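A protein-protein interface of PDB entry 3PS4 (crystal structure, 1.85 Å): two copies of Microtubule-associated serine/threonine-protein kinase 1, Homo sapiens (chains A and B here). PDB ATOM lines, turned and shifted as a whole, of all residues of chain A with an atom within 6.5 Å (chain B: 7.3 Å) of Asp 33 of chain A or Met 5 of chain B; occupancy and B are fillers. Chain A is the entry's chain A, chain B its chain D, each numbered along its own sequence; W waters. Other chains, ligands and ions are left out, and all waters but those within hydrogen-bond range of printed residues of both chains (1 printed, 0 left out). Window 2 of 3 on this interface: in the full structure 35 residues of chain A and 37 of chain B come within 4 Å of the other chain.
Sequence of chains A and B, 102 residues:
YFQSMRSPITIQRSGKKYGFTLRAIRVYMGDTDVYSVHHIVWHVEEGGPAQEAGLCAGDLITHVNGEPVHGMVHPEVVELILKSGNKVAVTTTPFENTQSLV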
ATOM      1  N   TYR A  28       8.129 -14.589  -4.644  1.00  0.00           N
ATOM      2  CA  TYR A  28       8.598 -13.411  -3.916  1.00  0.00           C
ATOM      3  C   TYR A  28      10.105 -13.279  -3.949  1.00  0.00           C
ATOM      4  O   TYR A  28      10.824 -14.286  -3.994  1.00  0.00           O
ATOM      5  CB  TYR A  28       8.097 -13.427  -2.471  1.00  0.00           C
ATOM      6  CG  TYR A  28       6.640 -13.040  -2.344  1.00  0.00           C
ATOM      7  CD1 TYR A  28       6.271 -11.737  -2.051  1.00  0.00           C
ATOM      8  CD2 TYR A  28       5.630 -13.977  -2.528  1.00  0.00           C
ATOM      9  CE1 TYR A  28       4.932 -11.370  -1.949  1.00  0.00           C
ATOM     10  CE2 TYR A  28       4.286 -13.619  -2.440  1.00  0.00           C
ATOM     11  CZ  TYR A  28       3.942 -12.313  -2.134  1.00  0.00           C
ATOM     12  OH  TYR A  28       2.628 -11.917  -2.035  1.00  0.00           O
ATOM     13  N   MET A  29      10.587 -12.027  -3.957  1.00  0.00           N
ATOM     14  CA  MET A  29      12.011 -11.733  -4.011  1.00  0.00           C
ATOM     15  C   MET A  29      12.577 -11.558  -2.611  1.00  0.00           C
ATOM     16  O   MET A  29      12.191 -10.635  -1.887  1.00  0.00           O
ATOM     17  CB  MET A  29      12.290 -10.491  -4.878  1.00  0.00           C
ATOM     18  CG  MET A  29      12.029 -10.721  -6.354  1.00  0.00           C
ATOM     19  SD  MET A  29      12.568  -9.347  -7.394  1.00  0.00           S
ATOM     20  CE  MET A  29      14.298  -9.761  -7.610  1.00  0.00           C
ATOM     21  N   ASP A  31      13.477 -11.301   1.063  1.00  0.00           N
ATOM     22  CA  ASP A  31      12.725 -11.009   2.289  1.00  0.00           C
ATOM     23  C   ASP A  31      11.643  -9.922   2.035  1.00  0.00           C
ATOM     24  O   ASP A  31      11.004  -9.475   2.980  1.00  0.00           O
ATOM     25  CB  ASP A  31      13.755 -10.539   3.360  1.00  0.00           C
ATOM     26  CG  ASP A  31      13.248 -10.292   4.774  1.00  0.00           C
ATOM     27  OD1 ASP A  31      12.761 -11.256   5.410  1.00  0.00           O
ATOM     28  OD2 ASP A  31      13.420  -9.156   5.277  1.00  0.00           O
ATOM     29  N   THR A  32      11.429  -9.515   0.769  1.00  0.00           N
ATOM     30  CA  THR A  32      10.510  -8.426   0.410  1.00  0.00           C
ATOM     31  C   THR A  32       9.097  -8.915   0.033  1.00  0.00           C
ATOM     32  O   THR A  32       8.866 -10.113  -0.125  1.00  0.00           O
ATOM     33  CB  THR A  32      11.089  -7.610  -0.769  1.00  0.00           C
ATOM     34  OG1 THR A  32      10.916  -8.364  -1.972  1.00  0.00           O
ATOM     35  CG2 THR A  32      12.565  -7.224  -0.584  1.00  0.00           C
ATOM     36  N   ASP A  33       8.172  -7.950  -0.156  1.00  0.00           N
ATOM     37  CA  ASP A  33       6.808  -8.214  -0.610  1.00  0.00           C
ATOM     38  C   ASP A  33       6.713  -8.024  -2.143  1.00  0.00           C
ATOM     39  O   ASP A  33       5.626  -7.965  -2.722  1.00  0.00           O
ATOM     40  CB  ASP A  33       5.777  -7.384   0.153  1.00  0.00           C
ATOM     41  CG  ASP A  33       5.389  -8.040   1.474  1.00  0.00           C
ATOM     42  OD1 ASP A  33       5.183  -9.282   1.490  1.00  0.00           O
ATOM     43  OD2 ASP A  33       5.351  -7.334   2.490  1.00  0.00           O
ATOM     44  N   VAL A  34       7.877  -7.993  -2.809  1.00  0.00           N
ATOM     45  CA  VAL A  34       7.958  -7.897  -4.266  1.00  0.00           C
ATOM     46  C   VAL A  34       7.832  -9.315  -4.841  1.00  0.00           C
ATOM     47  O   VAL A  34       8.546 -10.211  -4.387  1.00  0.00           O
ATOM     48  CB  VAL A  34       9.253  -7.201  -4.737  1.00  0.00           C
ATOM     49  CG1 VAL A  34       9.342  -7.153  -6.262  1.00  0.00           C
ATOM     50  CG2 VAL A  34       9.359  -5.801  -4.146  1.00  0.00           C
ATOM     51  N   TYR A  35       6.948  -9.518  -5.829  1.00  0.00           N
ATOM     52  CA  TYR A  35       6.798 -10.840  -6.450  1.00  0.00           C
ATOM     53  C   TYR A  35       6.489 -10.772  -7.953  1.00  0.00           C
ATOM     54  O   TYR A  35       6.049  -9.738  -8.460  1.00  0.00           O
ATOM     55  CB  TYR A  35       5.690 -11.657  -5.737  1.00  0.00           C
ATOM     56  CG  TYR A  35       4.286 -11.135  -5.949  1.00  0.00           C
ATOM     57  CD1 TYR A  35       3.503 -11.591  -7.011  1.00  0.00           C
ATOM     58  CD2 TYR A  35       3.737 -10.185  -5.087  1.00  0.00           C
ATOM     59  CE1 TYR A  35       2.216 -11.103  -7.219  1.00  0.00           C
ATOM     60  CE2 TYR A  35       2.444  -9.702  -5.276  1.00  0.00           C
ATOM     61  CZ  TYR A  35       1.685 -10.170  -6.339  1.00  0.00           C
ATOM     62  OH  TYR A  35       0.414  -9.689  -6.515  1.00  0.00           O
ATOM     63  N   SER B   4       7.709 -10.626   4.121  1.00  0.00           N
ATOM     64  CA  SER B   4       8.119  -9.377   4.785  1.00  0.00           C
ATOM     65  C   SER B   4       7.110  -8.995   5.868  1.00  0.00           C
ATOM     66  O   SER B   4       7.395  -9.154   7.062  1.00  0.00           O
ATOM     67  CB  SER B   4       8.255  -8.245   3.767  1.00  0.00           C
ATOM     68  N   MET B   5       5.919  -8.536   5.427  1.00  0.00           N
ATOM     69  CA  MET B   5       4.779  -8.140   6.243  1.00  0.00           C
ATOM     70  C   MET B   5       3.742  -9.288   6.351  1.00  0.00           C
ATOM     71  O   MET B   5       2.741  -9.155   7.057  1.00  0.00           O
ATOM     72  CB  MET B   5       4.124  -6.878   5.652  1.00  0.00           C
ATOM     73  CG  MET B   5       4.936  -5.597   5.868  1.00  0.00           C
ATOM     74  SD  MET B   5       5.039  -5.041   7.600  1.00  0.00           S
ATOM     75  CE  MET B   5       3.300  -4.570   7.902  1.00  0.00           C
ATOM     76  N   ARG B   6       3.996 -10.419   5.673  1.00  0.00           N
ATOM     77  CA  ARG B   6       3.096 -11.577   5.685  1.00  0.00           C
ATOM     78  C   ARG B   6       3.225 -12.320   7.027  1.00  0.00           C
ATOM     79  O   ARG B   6       4.333 -12.423   7.548  1.00  0.00           O
ATOM     80  CB  ARG B   6       3.382 -12.494   4.474  1.00  0.00           C
ATOM     81  CG  ARG B   6       2.805 -11.946   3.163  1.00  0.00           C
ATOM     82  CD  ARG B   6       3.279 -12.693   1.917  1.00  0.00           C
ATOM     83  NE  ARG B   6       4.665 -12.346   1.580  1.00  0.00           N
ATOM     84  CZ  ARG B   6       5.692 -13.191   1.648  1.00  0.00           C
ATOM     85  NH1 ARG B   6       5.492 -14.471   1.956  1.00  0.00           N
ATOM     86  NH2 ARG B   6       6.916 -12.776   1.367  1.00  0.00           N
ATOM     87  N   SER B   7       2.086 -12.773   7.614  1.00  0.00           N
ATOM     88  CA  SER B   7       2.051 -13.444   8.932  1.00  0.00           C
ATOM     89  C   SER B   7       2.453 -14.912   8.863  1.00  0.00           C
ATOM     90  O   SER B   7       1.880 -15.645   8.061  1.00  0.00           O
ATOM     91  CB  SER B   7       0.669 -13.359   9.567  1.00  0.00           C
ATOM     92  OG  SER B   7       0.170 -12.035   9.557  1.00  0.00           O
ATOM     93  N   PRO B   8       3.412 -15.373   9.701  1.00  0.00           N
ATOM     94  CA  PRO B   8       3.830 -16.783   9.616  1.00  0.00           C
ATOM     95  C   PRO B   8       2.815 -17.765  10.187  1.00  0.00           C
ATOM     96  O   PRO B   8       2.010 -17.410  11.034  1.00  0.00           O
ATOM     97  CB  PRO B   8       5.136 -16.830  10.416  1.00  0.00           C
ATOM     98  CG  PRO B   8       4.987 -15.736  11.409  1.00  0.00           C
ATOM     99  CD  PRO B   8       4.203 -14.633  10.710  1.00  0.00           C
ATOM    100  N   HIS B  63       9.982 -18.020   4.000  1.00  0.00           N
ATOM    101  CA  HIS B  63      10.804 -17.923   5.216  1.00  0.00           C
ATOM    102  C   HIS B  63      10.579 -19.098   6.136  1.00  0.00           C
ATOM    103  O   HIS B  63       9.464 -19.641   6.198  1.00  0.00           O
ATOM    104  CB  HIS B  63      10.503 -16.641   6.013  1.00  0.00           C
ATOM    105  CG  HIS B  63      10.706 -15.342   5.288  1.00  0.00           C
ATOM    106  ND1 HIS B  63       9.831 -14.921   4.301  1.00  0.00           N
ATOM    107  CD2 HIS B  63      11.601 -14.351   5.530  1.00  0.00           C
ATOM    108  CE1 HIS B  63      10.268 -13.731   3.923  1.00  0.00           C
ATOM    109  NE2 HIS B  63      11.312 -13.337   4.654  1.00  0.00           N
ATOM    110  N   THR B  91       6.706 -18.754   6.759  1.00  0.00           N
ATOM    111  CA  THR B  91       6.061 -17.640   6.083  1.00  0.00           C
ATOM    112  C   THR B  91       5.768 -18.098   4.676  1.00  0.00           C
ATOM    113  O   THR B  91       6.655 -18.648   4.021  1.00  0.00           O
ATOM    114  CB  THR B  91       6.918 -16.374   6.122  1.00  0.00           C
ATOM    115  OG1 THR B  91       7.356 -16.151   7.471  1.00  0.00           O
ATOM    116  CG2 THR B  91       6.171 -15.149   5.585  1.00  0.00           C
ATOM    117  N   THR B  92       4.536 -17.897   4.216  1.00  0.00           N
ATOM    118  CA  THR B  92       4.139 -18.379   2.894  1.00  0.00           C
ATOM    119  C   THR B  92       3.563 -17.292   2.017  1.00  0.00           C
ATOM    120  O   THR B  92       3.301 -16.180   2.482  1.00  0.00           O
ATOM    121  CB  THR B  92       3.065 -19.495   3.011  1.00  0.00           C
ATOM    122  OG1 THR B  92       1.853 -18.926   3.494  1.00  0.00           O
ATOM    123  CG2 THR B  92       3.494 -20.669   3.879  1.00  0.00           C
ATOM    124  N   PRO B  94       0.398 -15.634  -0.059  1.00  0.00           N
ATOM    125  CA  PRO B  94      -0.994 -15.539   0.445  1.00  0.00           C
ATOM    126  C   PRO B  94      -1.869 -16.679  -0.085  1.00  0.00           C
ATOM    127  O   PRO B  94      -1.521 -17.296  -1.098  1.00  0.00           O
ATOM    128  CB  PRO B  94      -1.470 -14.182  -0.072  1.00  0.00           C
ATOM    129  CG  PRO B  94      -0.191 -13.408  -0.345  1.00  0.00           C
ATOM    130  CD  PRO B  94       0.756 -14.447  -0.861  1.00  0.00           C
HETATM  131  O   HOH W   1       9.972 -12.780   0.893  1.00  0.00           O
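Water W1 lies within hydrogen-bond range of O of Thr 32 of chain A and NH2 of Arg 6 of chain B.
Of the 9 printed residues of chain B, 5 touch a printed residue of chain A. Hydrophobic or aromatic side chains of chain B within 4 Å of the printed part of chain A: Met 5, His 63 and Pro 94. Among the printed residues, Asp or Glu carboxylates within 4 Å of a Lys or Arg side-chain nitrogen of the other chain: Asp 33 of chain A with Arg 6 of chain B (3.1 Å).
Met 5 of chain B touches just one residue of chain A: Asp 33. Of the printed residues of chain B, Asp 31 of chain A touches Ser 4 and His 63. Printed residues of chain B within 4 Å of Thr 32 of chain A: Ser 4 (3.9 Å) and Arg 6 (3.6 Å). Of the printed residues of chain A, Arg 6 of chain B touches Tyr 28 (3.6 Å), Thr 32 (3.6 Å) and Asp 33 (3.1 Å). Of the printed residues of chain B, Tyr 28 of chain A touches Arg 6 and Pro 94. Of the printed residues of chain A, Ser 4 of chain B touches Asp 31 (3.1 Å), Thr 32 (3.9 Å) and Asp 33 (3.3 Å). Val 34 of chain A touches none of the printed residues of chain B. The nearest residue of chain B that does not touch Asp 33 of chain A is Pro 94 of chain B (7.0 Å). The nearest printed residue of chain B that does not touch Thr 32 of chain A is His 63 of chain B (5.4 Å).
The guanidinium group (NE) of Arg 6 of chain B lies within salt-bridge range of the side-chain carboxylate (OD1) of Asp 33 of chain A (3.1 Å). OD2 of Asp 33 of chain A lies within hydrogen-bond range of N of Met 5 of chain B, 3.2 Å away. The side-chain carboxylate of Asp 31 of chain A lies within hydrogen-bond range of a ring nitrogen (NE2) of His 63 of chain B, at 2.6 Å.
N of Thr 91 of chain B is in hydrogen-bond range of O of His 63 of chain B (3.0 Å). The guanidinium group of Arg 6 of chain B lies within hydrogen-bond range of the backbone carbonyl oxygen of Thr 92 of chain B, 2.8 Å away. The backbone NH of Val 34 of chain A is in hydrogen-bond range of the side-chain hydroxyl of Thr 32 of chain A (3.2 Å). The side-chain hydroxyl (OG1) of Thr 32 of chain A lies within hydrogen-bond range of the backbone carbonyl oxygen (O) of Met 29 of chain A (2.6 Å).
Among the printed residues, pairs that only touch across the chains: Tyr 28 of chain A with Arg 6 of chain B (3.6 Å), Tyr 28 of chain A with Pro 94 of chain B (3.4 Å), Asp 31 of chain A with Ser 4 of chain B (3.1 Å), Thr 32 of chain A with Ser 4 of chain B (3.9 Å), Thr 32 of chain A with Arg 6 of chain B (3.6 Å) and Asp 33 of chain A with Ser 4 of chain B (3.3 Å).
No position is printed for both chains. Of the 9 pairs that touch across the chains among the printed residues, none has its exchanged pair printed and touching as well.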
